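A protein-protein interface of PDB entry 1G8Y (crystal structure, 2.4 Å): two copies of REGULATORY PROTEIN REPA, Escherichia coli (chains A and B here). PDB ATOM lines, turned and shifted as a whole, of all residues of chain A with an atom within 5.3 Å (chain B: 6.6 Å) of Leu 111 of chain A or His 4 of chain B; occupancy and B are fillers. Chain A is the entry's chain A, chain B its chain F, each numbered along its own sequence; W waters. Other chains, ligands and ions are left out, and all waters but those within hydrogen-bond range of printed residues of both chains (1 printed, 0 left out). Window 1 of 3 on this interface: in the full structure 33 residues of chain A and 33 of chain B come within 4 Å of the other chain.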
ATOM      1  N   LEU A  74      11.290 -22.473 -29.174  1.00  0.00           N
ATOM      2  CA  LEU A  74      10.337 -22.492 -28.074  1.00  0.00           C
ATOM      3  C   LEU A  74       9.455 -23.743 -28.033  1.00  0.00           C
ATOM      4  O   LEU A  74       8.347 -23.753 -28.567  1.00  0.00           O
ATOM      5  CB  LEU A  74       9.455 -21.225 -28.133  1.00  0.00           C
ATOM      6  CG  LEU A  74      10.257 -19.911 -28.090  1.00  0.00           C
ATOM      7  CD1 LEU A  74       9.343 -18.695 -28.285  1.00  0.00           C
ATOM      8  CD2 LEU A  74      10.974 -19.833 -26.727  1.00  0.00           C
ATOM      9  N   PRO A  75       9.945 -24.814 -27.390  1.00  0.00           N
ATOM     10  CA  PRO A  75       9.166 -26.058 -27.291  1.00  0.00           C
ATOM     11  C   PRO A  75       8.198 -25.975 -26.120  1.00  0.00           C
ATOM     12  O   PRO A  75       8.604 -25.889 -24.962  1.00  0.00           O
ATOM     13  CB  PRO A  75      10.226 -27.134 -27.086  1.00  0.00           C
ATOM     14  CG  PRO A  75      11.341 -26.401 -26.355  1.00  0.00           C
ATOM     15  CD  PRO A  75      11.349 -25.005 -26.965  1.00  0.00           C
ATOM     16  N   ALA A  76       6.907 -26.002 -26.425  1.00  0.00           N
ATOM     17  CA  ALA A  76       5.895 -25.892 -25.389  1.00  0.00           C
ATOM     18  C   ALA A  76       5.167 -27.198 -25.136  1.00  0.00           C
ATOM     19  O   ALA A  76       4.234 -27.247 -24.330  1.00  0.00           O
ATOM     20  CB  ALA A  76       4.901 -24.812 -25.765  1.00  0.00           C
ATOM     21  N   PRO A  80      11.437 -30.737 -20.323  1.00  0.00           N
ATOM     22  CA  PRO A  80      12.853 -30.421 -20.520  1.00  0.00           C
ATOM     23  C   PRO A  80      13.751 -31.658 -20.663  1.00  0.00           C
ATOM     24  O   PRO A  80      14.677 -31.669 -21.481  1.00  0.00           O
ATOM     25  CB  PRO A  80      13.198 -29.581 -19.277  1.00  0.00           C
ATOM     26  CG  PRO A  80      11.899 -28.845 -19.029  1.00  0.00           C
ATOM     27  CD  PRO A  80      10.886 -29.983 -19.181  1.00  0.00           C
ATOM     28  N   GLN A 109      14.327 -22.183 -25.077  1.00  0.00           N
ATOM     29  CA  GLN A 109      13.596 -21.789 -23.870  1.00  0.00           C
ATOM     30  C   GLN A 109      12.333 -22.677 -23.734  1.00  0.00           C
ATOM     31  O   GLN A 109      11.369 -22.483 -24.438  1.00  0.00           O
ATOM     32  CB  GLN A 109      13.204 -20.301 -23.984  1.00  0.00           C
ATOM     33  CG  GLN A 109      12.240 -19.815 -22.896  1.00  0.00           C
ATOM     34  CD  GLN A 109      12.823 -20.066 -21.511  1.00  0.00           C
ATOM     35  OE1 GLN A 109      13.872 -19.521 -21.163  1.00  0.00           O
ATOM     36  NE2 GLN A 109      12.167 -20.894 -20.733  1.00  0.00           N
ATOM     37  N   PRO A 110      12.346 -23.675 -22.838  1.00  0.00           N
ATOM     38  CA  PRO A 110      11.167 -24.554 -22.677  1.00  0.00           C
ATOM     39  C   PRO A 110       9.952 -23.780 -22.181  1.00  0.00           C
ATOM     40  O   PRO A 110      10.091 -22.879 -21.352  1.00  0.00           O
ATOM     41  CB  PRO A 110      11.624 -25.598 -21.648  1.00  0.00           C
ATOM     42  CG  PRO A 110      13.125 -25.627 -21.842  1.00  0.00           C
ATOM     43  CD  PRO A 110      13.497 -24.169 -22.057  1.00  0.00           C
ATOM     44  N   LEU A 111       8.768 -24.139 -22.673  1.00  0.00           N
ATOM     45  CA  LEU A 111       7.550 -23.453 -22.283  1.00  0.00           C
ATOM     46  C   LEU A 111       6.387 -24.371 -21.978  1.00  0.00           C
ATOM     47  O   LEU A 111       5.238 -23.956 -22.018  1.00  0.00           O
ATOM     48  CB  LEU A 111       7.138 -22.471 -23.378  1.00  0.00           C
ATOM     49  CG  LEU A 111       8.000 -21.214 -23.634  1.00  0.00           C
ATOM     50  CD1 LEU A 111       7.353 -20.393 -24.756  1.00  0.00           C
ATOM     51  CD2 LEU A 111       8.120 -20.339 -22.340  1.00  0.00           C
ATOM     52  N   ILE A 112       6.664 -25.629 -21.676  1.00  0.00           N
ATOM     53  CA  ILE A 112       5.568 -26.546 -21.397  1.00  0.00           C
ATOM     54  C   ILE A 112       4.870 -26.118 -20.101  1.00  0.00           C
ATOM     55  O   ILE A 112       5.506 -25.909 -19.062  1.00  0.00           O
ATOM     56  CB  ILE A 112       6.087 -28.006 -21.309  1.00  0.00           C
ATOM     57  CG1 ILE A 112       4.915 -28.974 -21.203  1.00  0.00           C
ATOM     58  CG2 ILE A 112       7.070 -28.155 -20.149  1.00  0.00           C
ATOM     59  CD1 ILE A 112       5.331 -30.470 -21.261  1.00  0.00           C
ATOM     60  N   GLY A 113       3.558 -25.964 -20.174  1.00  0.00           N
ATOM     61  CA  GLY A 113       2.807 -25.545 -19.010  1.00  0.00           C
ATOM     62  C   GLY A 113       3.006 -24.074 -18.690  1.00  0.00           C
ATOM     63  O   GLY A 113       2.602 -23.634 -17.625  1.00  0.00           O
ATOM     64  N   SER A 114       3.647 -23.325 -19.593  1.00  0.00           N
ATOM     65  CA  SER A 114       3.884 -21.901 -19.383  1.00  0.00           C
ATOM     66  C   SER A 114       2.707 -21.082 -19.909  1.00  0.00           C
ATOM     67  O   SER A 114       2.569 -19.915 -19.581  1.00  0.00           O
ATOM     68  CB  SER A 114       5.161 -21.435 -20.083  1.00  0.00           C
ATOM     69  OG  SER A 114       6.277 -22.168 -19.629  1.00  0.00           O
ATOM     70  N   LEU A 115       1.874 -21.711 -20.727  1.00  0.00           N
ATOM     71  CA  LEU A 115       0.681 -21.081 -21.283  1.00  0.00           C
ATOM     72  C   LEU A 115       0.870 -19.780 -22.059  1.00  0.00           C
ATOM     73  O   LEU A 115       0.211 -18.794 -21.797  1.00  0.00           O
ATOM     74  CB  LEU A 115      -0.341 -20.886 -20.168  1.00  0.00           C
ATOM     75  CG  LEU A 115      -0.531 -22.185 -19.377  1.00  0.00           C
ATOM     76  CD1 LEU A 115      -1.544 -21.998 -18.251  1.00  0.00           C
ATOM     77  CD2 LEU A 115      -0.963 -23.285 -20.327  1.00  0.00           C
ATOM     78  N   PRO A 116       1.778 -19.775 -23.043  1.00  0.00           N
ATOM     79  CA  PRO A 116       1.975 -18.541 -23.814  1.00  0.00           C
ATOM     80  C   PRO A 116       0.688 -18.221 -24.601  1.00  0.00           C
ATOM     81  O   PRO A 116      -0.014 -19.124 -25.069  1.00  0.00           O
ATOM     82  CB  PRO A 116       3.125 -18.881 -24.775  1.00  0.00           C
ATOM     83  CG  PRO A 116       3.660 -20.208 -24.306  1.00  0.00           C
ATOM     84  CD  PRO A 116       2.563 -20.897 -23.584  1.00  0.00           C
ATOM     85  N   TRP A 123       2.692 -11.482 -23.374  1.00  0.00           N
ATOM     86  CA  TRP A 123       3.327 -12.503 -24.202  1.00  0.00           C
ATOM     87  C   TRP A 123       3.678 -11.976 -25.595  1.00  0.00           C
ATOM     88  O   TRP A 123       4.730 -12.309 -26.142  1.00  0.00           O
ATOM     89  CB  TRP A 123       2.455 -13.755 -24.308  1.00  0.00           C
ATOM     90  CG  TRP A 123       2.657 -14.669 -23.171  1.00  0.00           C
ATOM     91  CD1 TRP A 123       1.792 -14.903 -22.150  1.00  0.00           C
ATOM     92  CD2 TRP A 123       3.826 -15.456 -22.901  1.00  0.00           C
ATOM     93  NE1 TRP A 123       2.343 -15.783 -21.253  1.00  0.00           N
ATOM     94  CE2 TRP A 123       3.590 -16.145 -21.688  1.00  0.00           C
ATOM     95  CE3 TRP A 123       5.048 -15.650 -23.568  1.00  0.00           C
ATOM     96  CZ2 TRP A 123       4.534 -17.027 -21.124  1.00  0.00           C
ATOM     97  CZ3 TRP A 123       6.000 -16.533 -23.002  1.00  0.00           C
ATOM     98  CH2 TRP A 123       5.730 -17.204 -21.799  1.00  0.00           C
ATOM     99  N   PHE A 145       0.388 -21.538 -28.341  1.00  0.00           N
ATOM    100  CA  PHE A 145       0.695 -20.122 -28.264  1.00  0.00           C
ATOM    101  C   PHE A 145      -0.512 -19.211 -28.445  1.00  0.00           C
ATOM    102  O   PHE A 145      -0.376 -17.995 -28.548  1.00  0.00           O
ATOM    103  CB  PHE A 145       1.793 -19.757 -29.274  1.00  0.00           C
ATOM    104  CG  PHE A 145       3.143 -20.310 -28.916  1.00  0.00           C
ATOM    105  CD1 PHE A 145       3.450 -21.643 -29.145  1.00  0.00           C
ATOM    106  CD2 PHE A 145       4.102 -19.500 -28.317  1.00  0.00           C
ATOM    107  CE1 PHE A 145       4.697 -22.165 -28.784  1.00  0.00           C
ATOM    108  CE2 PHE A 145       5.363 -20.012 -27.944  1.00  0.00           C
ATOM    109  CZ  PHE A 145       5.656 -21.331 -28.176  1.00  0.00           C
ATOM    110  N   ALA B   2       3.733 -22.699 -15.258  1.00  0.00           N
ATOM    111  CA  ALA B   2       5.049 -23.217 -14.914  1.00  0.00           C
ATOM    112  C   ALA B   2       6.133 -22.459 -15.725  1.00  0.00           C
ATOM    113  O   ALA B   2       5.850 -21.899 -16.783  1.00  0.00           O
ATOM    114  CB  ALA B   2       5.097 -24.744 -15.199  1.00  0.00           C
ATOM    115  N   THR B   3       7.355 -22.400 -15.207  1.00  0.00           N
ATOM    116  CA  THR B   3       8.440 -21.711 -15.900  1.00  0.00           C
ATOM    117  C   THR B   3       9.592 -22.680 -16.026  1.00  0.00           C
ATOM    118  O   THR B   3       9.621 -23.722 -15.369  1.00  0.00           O
ATOM    119  CB  THR B   3       8.933 -20.480 -15.117  1.00  0.00           C
ATOM    120  OG1 THR B   3       9.374 -20.887 -13.811  1.00  0.00           O
ATOM    121  CG2 THR B   3       7.814 -19.454 -14.990  1.00  0.00           C
ATOM    122  N   HIS B   4      10.557 -22.347 -16.865  1.00  0.00           N
ATOM    123  CA  HIS B   4      11.701 -23.236 -17.031  1.00  0.00           C
ATOM    124  C   HIS B   4      12.921 -22.391 -17.350  1.00  0.00           C
ATOM    125  O   HIS B   4      12.840 -21.328 -17.977  1.00  0.00           O
ATOM    126  CB  HIS B   4      11.464 -24.227 -18.202  1.00  0.00           C
ATOM    127  CG  HIS B   4      10.128 -24.916 -18.168  1.00  0.00           C
ATOM    128  ND1 HIS B   4       9.889 -26.046 -17.415  1.00  0.00           N
ATOM    129  CD2 HIS B   4       8.952 -24.607 -18.762  1.00  0.00           C
ATOM    130  CE1 HIS B   4       8.624 -26.399 -17.540  1.00  0.00           C
ATOM    131  NE2 HIS B   4       8.029 -25.542 -18.352  1.00  0.00           N
ATOM    132  N   LYS B   5      14.072 -22.850 -16.915  1.00  0.00           N
ATOM    133  CA  LYS B   5      15.252 -22.113 -17.282  1.00  0.00           C
ATOM    134  C   LYS B   5      15.694 -22.590 -18.677  1.00  0.00           C
ATOM    135  O   LYS B   5      15.337 -23.698 -19.126  1.00  0.00           O
ATOM    136  CB  LYS B   5      16.367 -22.353 -16.272  1.00  0.00           C
ATOM    137  CG  LYS B   5      16.564 -23.788 -15.917  1.00  0.00           C
ATOM    138  CD  LYS B   5      17.829 -24.338 -16.523  1.00  0.00           C
ATOM    139  CE  LYS B   5      18.245 -25.570 -15.741  1.00  0.00           C
ATOM    140  NZ  LYS B   5      17.088 -26.514 -15.545  1.00  0.00           N
ATOM    141  N   PRO B   6      16.445 -21.738 -19.384  1.00  0.00           N
ATOM    142  CA  PRO B   6      16.954 -22.052 -20.708  1.00  0.00           C
ATOM    143  C   PRO B   6      17.731 -23.362 -20.609  1.00  0.00           C
ATOM    144  O   PRO B   6      18.340 -23.640 -19.586  1.00  0.00           O
ATOM    145  CB  PRO B   6      17.893 -20.875 -20.994  1.00  0.00           C
ATOM    146  CG  PRO B   6      17.217 -19.744 -20.306  1.00  0.00           C
ATOM    147  CD  PRO B   6      16.825 -20.365 -18.986  1.00  0.00           C
ATOM    148  N   ALA B 168       3.789 -29.801 -15.047  1.00  0.00           N
ATOM    149  CA  ALA B 168       5.157 -29.292 -15.154  1.00  0.00           C
ATOM    150  C   ALA B 168       5.618 -28.619 -13.862  1.00  0.00           C
ATOM    151  O   ALA B 168       6.784 -28.700 -13.486  1.00  0.00           O
ATOM    152  CB  ALA B 168       5.272 -28.321 -16.339  1.00  0.00           C
ATOM    153  N   ASP B 169       4.695 -27.974 -13.165  1.00  0.00           N
ATOM    154  CA  ASP B 169       5.044 -27.305 -11.934  1.00  0.00           C
ATOM    155  C   ASP B 169       5.351 -28.253 -10.754  1.00  0.00           C
ATOM    156  O   ASP B 169       6.348 -28.097 -10.036  1.00  0.00           O
ATOM    157  CB  ASP B 169       3.911 -26.366 -11.549  1.00  0.00           C
ATOM    158  CG  ASP B 169       4.404 -25.160 -10.837  1.00  0.00           C
ATOM    159  OD1 ASP B 169       5.067 -24.324 -11.478  1.00  0.00           O
ATOM    160  OD2 ASP B 169       4.150 -25.055  -9.623  1.00  0.00           O
HETATM  161  O   HOH W   1       4.385 -18.805 -17.478  1.00  0.00           O
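The backbone carbonyl oxygen (O) of Ile 112 of chain A sits at hydrogen-bond distance from a ring nitrogen (NE2) of His 4 of chain B (2.6 Å). O of Gly 113 of chain A lies within hydrogen-bond range of N of Ala 2 of chain B (2.8 Å). OG of Ser 114 of chain A is in hydrogen-bond range of O of Ala 2 of chain B (2.9 Å). The backbone carbonyl oxygen of His 4 of chain B lies within hydrogen-bond range of the side-chain amide nitrogen of Gln 109 of chain A (2.9 Å).
The backbone carbonyl oxygen (O) of Leu 111 of chain A is in hydrogen-bond range of the side-chain hydroxyl (OG) of Ser 114 of chain A (3.2 Å). O of Pro 75 of chain A is in hydrogen-bond range of N of Leu 111 of chain A, 2.9 Å away.
Among the printed residues, pairs that only touch across the chains: Pro 80 of chain A with His 4 of chain B (3.8 Å), Gln 109 of chain A with Pro 6 of chain B (3.5 Å), Pro 110 of chain A with His 4 of chain B (3.3 Å), Pro 110 of chain A with Lys 5 of chain B (3.5 Å), Leu 111 of chain A with His 4 of chain B (3.9 Å), Ile 112 of chain A with Ala 168 of chain B (3.6 Å) and Ser 114 of chain A with His 4 of chain B (3.7 Å).
Of chain B, only His 4 comes within 4 Å of Leu 111 of chain A. Printed residues of chain A within 4 Å of His 4 of chain B: Pro 80, Gln 109, Pro 110, Leu 111, Ile 112 and Ser 114. Of the printed residues of chain A, Pro 6 of chain B touches Gln 109 (3.5 Å). Printed residues of chain A within 4 Å of Lys 5 of chain B: Pro 110. Printed residues of chain B within 4 Å of Pro 110 of chain A: His 4 (3.3 Å) and Lys 5 (3.5 Å). Of the printed residues of chain B, Gly 113 of chain A touches Ala 2 (2.8 Å). Of the printed residues of chain A, Ala 2 of chain B touches Gly 113 and Ser 114. The nearest residue of chain A that does not touch His 4 of chain B is Gly 113 of chain A (4.8 Å).
Hydrophobic or aromatic side chains of chain A within 4 Å of the printed part of chain B: Pro 80, Pro 110 and Ile 112. Of the 7 printed residues of chain B, 5 touch a printed residue of chain A. Among the printed residues, 11 pairs touch across the chains. Among the printed residues, no Asp or Glu carboxylate lies within 4 Å of a Lys or Arg side-chain nitrogen of the other chain.
No position is printed for both chains. Of the 11 pairs that touch across the chains among the printed residues, none has its exchanged pair printed and touching as well.
Water W1 bridges the backbone carbonyl oxygen (O) of Ser 114 of chain A (3.0 Å) and the backbone carbonyl oxygen (O) of Ala 2 of chain B (3.5 Å).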
